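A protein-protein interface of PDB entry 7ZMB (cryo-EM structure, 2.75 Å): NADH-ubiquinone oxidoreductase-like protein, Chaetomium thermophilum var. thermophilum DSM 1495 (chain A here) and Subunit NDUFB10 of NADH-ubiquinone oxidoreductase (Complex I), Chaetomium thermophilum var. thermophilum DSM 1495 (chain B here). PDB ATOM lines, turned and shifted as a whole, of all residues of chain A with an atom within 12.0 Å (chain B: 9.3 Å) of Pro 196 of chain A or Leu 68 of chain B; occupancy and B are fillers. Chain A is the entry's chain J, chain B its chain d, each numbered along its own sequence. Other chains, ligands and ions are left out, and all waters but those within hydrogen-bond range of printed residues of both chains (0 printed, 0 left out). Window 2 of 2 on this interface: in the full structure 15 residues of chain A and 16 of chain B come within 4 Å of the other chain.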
ATOM      1  N   PRO A 191     -28.939  30.835   2.866  1.00  0.00           N
ATOM      2  CA  PRO A 191     -27.802  30.081   2.330  1.00  0.00           C
ATOM      3  C   PRO A 191     -26.479  30.649   2.820  1.00  0.00           C
ATOM      4  O   PRO A 191     -26.338  31.854   3.044  1.00  0.00           O
ATOM      5  CB  PRO A 191     -27.954  30.235   0.814  1.00  0.00           C
ATOM      6  CG  PRO A 191     -29.392  30.585   0.607  1.00  0.00           C
ATOM      7  CD  PRO A 191     -29.783  31.397   1.799  1.00  0.00           C
ATOM      8  N   VAL A 192     -25.503  29.756   2.988  1.00  0.00           N
ATOM      9  CA  VAL A 192     -24.224  30.134   3.573  1.00  0.00           C
ATOM     10  C   VAL A 192     -23.504  31.133   2.675  1.00  0.00           C
ATOM     11  O   VAL A 192     -23.663  31.136   1.447  1.00  0.00           O
ATOM     12  CB  VAL A 192     -23.354  28.888   3.820  1.00  0.00           C
ATOM     13  CG1 VAL A 192     -23.910  28.080   4.979  1.00  0.00           C
ATOM     14  CG2 VAL A 192     -23.280  28.042   2.563  1.00  0.00           C
ATOM     15  N   CYS A 193     -22.700  31.997   3.302  1.00  0.00           N
ATOM     16  CA  CYS A 193     -21.969  33.011   2.551  1.00  0.00           C
ATOM     17  C   CYS A 193     -20.941  32.377   1.621  1.00  0.00           C
ATOM     18  O   CYS A 193     -20.569  32.973   0.607  1.00  0.00           O
ATOM     19  CB  CYS A 193     -21.295  33.992   3.509  1.00  0.00           C
ATOM     20  SG  CYS A 193     -20.378  35.321   2.696  1.00  0.00           S
ATOM     21  N   ALA A 194     -20.443  31.190   1.976  1.00  0.00           N
ATOM     22  CA  ALA A 194     -19.644  30.336   1.089  1.00  0.00           C
ATOM     23  C   ALA A 194     -18.458  31.066   0.460  1.00  0.00           C
ATOM     24  O   ALA A 194     -18.055  30.755  -0.664  1.00  0.00           O
ATOM     25  CB  ALA A 194     -20.515  29.716  -0.007  1.00  0.00           C
ATOM     26  N   ASP A 195     -17.875  32.030   1.175  1.00  0.00           N
ATOM     27  CA  ASP A 195     -16.740  32.768   0.648  1.00  0.00           C
ATOM     28  C   ASP A 195     -15.912  33.357   1.781  1.00  0.00           C
ATOM     29  O   ASP A 195     -16.469  33.959   2.712  1.00  0.00           O
ATOM     30  CB  ASP A 195     -17.193  33.894  -0.290  1.00  0.00           C
ATOM     31  CG  ASP A 195     -16.120  34.288  -1.280  1.00  0.00           C
ATOM     32  OD1 ASP A 195     -15.502  33.382  -1.877  1.00  0.00           O
ATOM     33  OD2 ASP A 195     -15.890  35.502  -1.458  1.00  0.00           O
ATOM     34  N   PRO A 196     -14.586  33.195   1.735  1.00  0.00           N
ATOM     35  CA  PRO A 196     -13.741  33.847   2.750  1.00  0.00           C
ATOM     36  C   PRO A 196     -13.895  35.356   2.766  1.00  0.00           C
ATOM     37  O   PRO A 196     -13.861  35.970   3.841  1.00  0.00           O
ATOM     38  CB  PRO A 196     -12.323  33.420   2.345  1.00  0.00           C
ATOM     39  CG  PRO A 196     -12.513  32.174   1.547  1.00  0.00           C
ATOM     40  CD  PRO A 196     -13.801  32.365   0.809  1.00  0.00           C
ATOM     41  N   ASP A 197     -14.063  35.973   1.601  1.00  0.00           N
ATOM     42  CA  ASP A 197     -14.295  37.403   1.523  1.00  0.00           C
ATOM     43  C   ASP A 197     -15.789  37.692   1.424  1.00  0.00           C
ATOM     44  O   ASP A 197     -16.614  36.787   1.275  1.00  0.00           O
ATOM     45  CB  ASP A 197     -13.561  38.007   0.326  1.00  0.00           C
ATOM     46  N   GLN A 198     -16.127  38.977   1.514  1.00  0.00           N
ATOM     47  CA  GLN A 198     -17.511  39.441   1.431  1.00  0.00           C
ATOM     48  C   GLN A 198     -18.399  38.765   2.472  1.00  0.00           C
ATOM     49  O   GLN A 198     -19.555  38.441   2.199  1.00  0.00           O
ATOM     50  CB  GLN A 198     -18.077  39.204   0.028  1.00  0.00           C
ATOM     51  N   CYS B  59      -7.423  25.896 -10.163  1.00  0.00           N
ATOM     52  CA  CYS B  59      -6.990  26.252  -8.815  1.00  0.00           C
ATOM     53  C   CYS B  59      -6.941  25.042  -7.897  1.00  0.00           C
ATOM     54  O   CYS B  59      -6.010  24.907  -7.097  1.00  0.00           O
ATOM     55  CB  CYS B  59      -7.898  27.316  -8.202  1.00  0.00           C
ATOM     56  SG  CYS B  59      -7.871  28.949  -8.923  1.00  0.00           S
ATOM     57  N   TYR B  60      -7.942  24.165  -7.979  1.00  0.00           N
ATOM     58  CA  TYR B  60      -8.044  23.080  -7.014  1.00  0.00           C
ATOM     59  C   TYR B  60      -6.793  22.218  -6.996  1.00  0.00           C
ATOM     60  O   TYR B  60      -6.369  21.748  -5.933  1.00  0.00           O
ATOM     61  CB  TYR B  60      -9.258  22.208  -7.302  1.00  0.00           C
ATOM     62  CG  TYR B  60      -9.377  21.133  -6.263  1.00  0.00           C
ATOM     63  CD1 TYR B  60      -9.688  21.458  -4.959  1.00  0.00           C
ATOM     64  CD2 TYR B  60      -9.118  19.804  -6.569  1.00  0.00           C
ATOM     65  CE1 TYR B  60      -9.777  20.497  -3.996  1.00  0.00           C
ATOM     66  CE2 TYR B  60      -9.210  18.832  -5.605  1.00  0.00           C
ATOM     67  CZ  TYR B  60      -9.539  19.190  -4.316  1.00  0.00           C
ATOM     68  OH  TYR B  60      -9.641  18.246  -3.329  1.00  0.00           O
ATOM     69  N   GLU B  63      -3.606  24.599  -5.654  1.00  0.00           N
ATOM     70  CA  GLU B  63      -3.536  24.958  -4.246  1.00  0.00           C
ATOM     71  C   GLU B  63      -3.593  23.754  -3.322  1.00  0.00           C
ATOM     72  O   GLU B  63      -2.742  23.613  -2.439  1.00  0.00           O
ATOM     73  CB  GLU B  63      -4.659  25.944  -3.899  1.00  0.00           C
ATOM     74  CG  GLU B  63      -4.481  27.315  -4.532  1.00  0.00           C
ATOM     75  CD  GLU B  63      -3.027  27.752  -4.593  1.00  0.00           C
ATOM     76  OE1 GLU B  63      -2.340  27.723  -3.550  1.00  0.00           O
ATOM     77  OE2 GLU B  63      -2.567  28.120  -5.694  1.00  0.00           O
ATOM     78  N   GLY B  64      -4.576  22.880  -3.493  1.00  0.00           N
ATOM     79  CA  GLY B  64      -4.615  21.663  -2.713  1.00  0.00           C
ATOM     80  C   GLY B  64      -5.088  21.869  -1.291  1.00  0.00           C
ATOM     81  O   GLY B  64      -6.280  22.081  -1.046  1.00  0.00           O
ATOM     82  N   VAL B  65      -4.154  21.793  -0.340  1.00  0.00           N
ATOM     83  CA  VAL B  65      -4.495  22.003   1.064  1.00  0.00           C
ATOM     84  C   VAL B  65      -5.103  23.384   1.266  1.00  0.00           C
ATOM     85  O   VAL B  65      -6.165  23.530   1.884  1.00  0.00           O
ATOM     86  CB  VAL B  65      -3.255  21.794   1.948  1.00  0.00           C
ATOM     87  CG1 VAL B  65      -3.453  22.431   3.296  1.00  0.00           C
ATOM     88  CG2 VAL B  65      -3.011  20.320   2.132  1.00  0.00           C
ATOM     89  N   ASN B  66      -4.446  24.415   0.751  1.00  0.00           N
ATOM     90  CA  ASN B  66      -4.968  25.775   0.859  1.00  0.00           C
ATOM     91  C   ASN B  66      -5.809  26.176  -0.353  1.00  0.00           C
ATOM     92  O   ASN B  66      -5.664  27.259  -0.916  1.00  0.00           O
ATOM     93  CB  ASN B  66      -3.811  26.742   1.105  1.00  0.00           C
ATOM     94  CG  ASN B  66      -2.885  26.892  -0.095  1.00  0.00           C
ATOM     95  OD1 ASN B  66      -3.109  26.316  -1.159  1.00  0.00           O
ATOM     96  ND2 ASN B  66      -1.826  27.674   0.081  1.00  0.00           N
ATOM     97  N   HIS B  67      -6.767  25.321  -0.721  1.00  0.00           N
ATOM     98  CA  HIS B  67      -7.674  25.608  -1.864  1.00  0.00           C
ATOM     99  C   HIS B  67      -8.951  26.277  -1.360  1.00  0.00           C
ATOM    100  O   HIS B  67      -9.604  26.968  -2.154  1.00  0.00           O
ATOM    101  CB  HIS B  67      -8.004  24.319  -2.622  1.00  0.00           C
ATOM    102  CG  HIS B  67      -9.133  23.526  -2.053  1.00  0.00           C
ATOM    103  ND1 HIS B  67     -10.420  23.618  -2.543  1.00  0.00           N
ATOM    104  CD2 HIS B  67      -9.178  22.618  -1.057  1.00  0.00           C
ATOM    105  CE1 HIS B  67     -11.205  22.803  -1.871  1.00  0.00           C
ATOM    106  NE2 HIS B  67     -10.466  22.177  -0.957  1.00  0.00           N
ATOM    107  N   LEU B  68      -9.279  26.077  -0.084  1.00  0.00           N
ATOM    108  CA  LEU B  68     -10.507  26.640   0.446  1.00  0.00           C
ATOM    109  C   LEU B  68     -10.379  28.117   0.768  1.00  0.00           C
ATOM    110  O   LEU B  68     -11.375  28.737   1.151  1.00  0.00           O
ATOM    111  CB  LEU B  68     -10.936  25.856   1.683  1.00  0.00           C
ATOM    112  CG  LEU B  68     -11.396  24.435   1.370  1.00  0.00           C
ATOM    113  CD1 LEU B  68     -11.500  23.598   2.629  1.00  0.00           C
ATOM    114  CD2 LEU B  68     -12.730  24.476   0.647  1.00  0.00           C
ATOM    115  N   GLU B  69      -9.190  28.701   0.607  1.00  0.00           N
ATOM    116  CA  GLU B  69      -9.001  30.104   0.945  1.00  0.00           C
ATOM    117  C   GLU B  69      -8.212  30.882  -0.100  1.00  0.00           C
ATOM    118  O   GLU B  69      -7.759  31.994   0.197  1.00  0.00           O
ATOM    119  CB  GLU B  69      -8.313  30.234   2.310  1.00  0.00           C
ATOM    120  CG  GLU B  69      -6.860  29.801   2.325  1.00  0.00           C
ATOM    121  CD  GLU B  69      -6.085  30.419   3.474  1.00  0.00           C
ATOM    122  OE1 GLU B  69      -6.560  31.428   4.036  1.00  0.00           O
ATOM    123  OE2 GLU B  69      -5.004  29.896   3.815  1.00  0.00           O
ATOM    124  N   LYS B  70      -8.036  30.356  -1.306  1.00  0.00           N
ATOM    125  CA  LYS B  70      -7.321  31.098  -2.338  1.00  0.00           C
ATOM    126  C   LYS B  70      -8.107  31.256  -3.629  1.00  0.00           C
ATOM    127  O   LYS B  70      -8.039  32.314  -4.258  1.00  0.00           O
ATOM    128  CB  LYS B  70      -5.973  30.425  -2.628  1.00  0.00           C
ATOM    129  CG  LYS B  70      -4.920  30.729  -1.575  1.00  0.00           C
ATOM    130  CD  LYS B  70      -3.573  30.142  -1.943  1.00  0.00           C
ATOM    131  CE  LYS B  70      -2.910  30.932  -3.055  1.00  0.00           C
ATOM    132  NZ  LYS B  70      -1.595  30.346  -3.436  1.00  0.00           N
ATOM    133  N   CYS B  71      -8.856  30.236  -4.042  1.00  0.00           N
ATOM    134  CA  CYS B  71      -9.786  30.374  -5.158  1.00  0.00           C
ATOM    135  C   CYS B  71     -11.197  29.984  -4.749  1.00  0.00           C
ATOM    136  O   CYS B  71     -11.803  29.099  -5.357  1.00  0.00           O
ATOM    137  CB  CYS B  71      -9.351  29.549  -6.375  1.00  0.00           C
ATOM    138  SG  CYS B  71      -7.853  30.091  -7.240  1.00  0.00           S
ATOM    139  N   GLY B  72     -11.716  30.616  -3.701  1.00  0.00           N
ATOM    140  CA  GLY B  72     -13.128  30.518  -3.394  1.00  0.00           C
ATOM    141  C   GLY B  72     -13.946  31.542  -4.150  1.00  0.00           C
ATOM    142  O   GLY B  72     -15.169  31.428  -4.242  1.00  0.00           O
ATOM    143  N   LYS B  73     -13.278  32.565  -4.686  1.00  0.00           N
ATOM    144  CA  LYS B  73     -13.982  33.571  -5.474  1.00  0.00           C
ATOM    145  C   LYS B  73     -14.512  32.973  -6.768  1.00  0.00           C
ATOM    146  O   LYS B  73     -15.663  33.212  -7.150  1.00  0.00           O
ATOM    147  CB  LYS B  73     -13.058  34.753  -5.765  1.00  0.00           C
ATOM    148  CG  LYS B  73     -13.651  35.771  -6.722  1.00  0.00           C
ATOM    149  CD  LYS B  73     -12.762  36.994  -6.846  1.00  0.00           C
ATOM    150  CE  LYS B  73     -13.216  37.884  -7.988  1.00  0.00           C
ATOM    151  NZ  LYS B  73     -13.065  37.205  -9.304  1.00  0.00           N
ATOM    152  N   LEU B  74     -13.740  32.074  -7.385  1.00  0.00           N
ATOM    153  CA  LEU B  74     -14.289  31.381  -8.583  1.00  0.00           C
ATOM    154  C   LEU B  74     -15.385  30.405  -8.161  1.00  0.00           C
ATOM    155  O   LEU B  74     -16.267  30.111  -8.988  1.00  0.00           O
ATOM    156  CB  LEU B  74     -13.143  30.614  -9.255  1.00  0.00           C
ATOM    157  CG  LEU B  74     -12.387  31.343 -10.364  1.00  0.00           C
ATOM    158  CD1 LEU B  74     -12.003  32.755  -9.945  1.00  0.00           C
ATOM    159  CD2 LEU B  74     -11.148  30.560 -10.762  1.00  0.00           C
ATOM    160  N   ARG B  75     -15.348  29.952  -6.914  1.00  0.00           N
ATOM    161  CA  ARG B  75     -16.308  28.917  -6.453  1.00  0.00           C
ATOM    162  C   ARG B  75     -17.712  29.500  -6.381  1.00  0.00           C
ATOM    163  O   ARG B  75     -18.658  28.825  -6.808  1.00  0.00           O
ATOM    164  CB  ARG B  75     -15.867  28.423  -5.077  1.00  0.00           C
ATOM    165  CG  ARG B  75     -16.356  27.031  -4.724  1.00  0.00           C
ATOM    166  CD  ARG B  75     -15.854  26.674  -3.349  1.00  0.00           C
ATOM    167  NE  ARG B  75     -14.434  26.367  -3.287  1.00  0.00           N
ATOM    168  CZ  ARG B  75     -13.567  26.973  -2.487  1.00  0.00           C
ATOM    169  NH1 ARG B  75     -12.296  26.617  -2.502  1.00  0.00           N
ATOM    170  NH2 ARG B  75     -13.971  27.929  -1.670  1.00  0.00           N
ATOM    171  N   GLU B  76     -17.824  30.712  -5.845  1.00  0.00           N
ATOM    172  CA  GLU B  76     -19.149  31.353  -5.685  1.00  0.00           C
ATOM    173  C   GLU B  76     -19.738  31.587  -7.073  1.00  0.00           C
ATOM    174  O   GLU B  76     -20.952  31.396  -7.236  1.00  0.00           O
ATOM    175  CB  GLU B  76     -19.035  32.633  -4.858  1.00  0.00           C
ATOM    176  CG  GLU B  76     -19.557  32.482  -3.441  1.00  0.00           C
ATOM    177  CD  GLU B  76     -21.071  32.477  -3.314  1.00  0.00           C
ATOM    178  OE1 GLU B  76     -21.569  32.142  -2.223  1.00  0.00           O
ATOM    179  OE2 GLU B  76     -21.749  32.818  -4.304  1.00  0.00           O
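The backbone carbonyl oxygen (O) of Cys 193 of chain A sits close to the side-chain carboxylate (OE1) of Glu 76 of chain B (3.1 Å).
The side-chain carboxylate of Asp 195 of chain A sits close to the backbone carbonyl oxygen of Gly 72 of chain B.
The side-chain sulfur of Cys 193 of chain A is in hydrogen-bond range of the backbone carbonyl oxygen of Gln 198 of chain A (3.3 Å).
SG of Cys 59 of chain B is disulfide-bonded to SG of Cys 71 of chain B.
OE1 of Glu 76 of chain B touches CB of Ala 194 of chain A, at 3.5 Å.
N of Lys 73 of chain B touches OD1 of Asp 195 of chain A (3.7 Å).
Pro 196 of chain A touches Leu 68 of chain B.
Of the printed residues of chain B, Cys 193 of chain A touches Glu 76 (3.1 Å).
Printed residues of chain B within 4 Å of Pro 196 of chain A: Leu 68.
No residue of chain A comes within 4 Å of Gly 64 of chain B.
Asn 66 of chain B touches none of the printed residues of chain A.
No residue of chain A comes within 4 Å of His 67 of chain B.
No residue of chain A comes within 4 Å of Glu 69 of chain B.
Lys 70 of chain B touches none of the printed residues of chain A.
Of the printed residues of chain A, Lys 73 of chain B touches Asp 195.
The nearest residue of chain B that does not touch Pro 196 of chain A is Glu 69 of chain B (4.1 Å).
The nearest residue of chain A that does not touch Leu 68 of chain B is Asp 195 of chain A (6.5 Å).
Of the 16 printed residues of chain B, 4 touch a printed residue of chain A.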
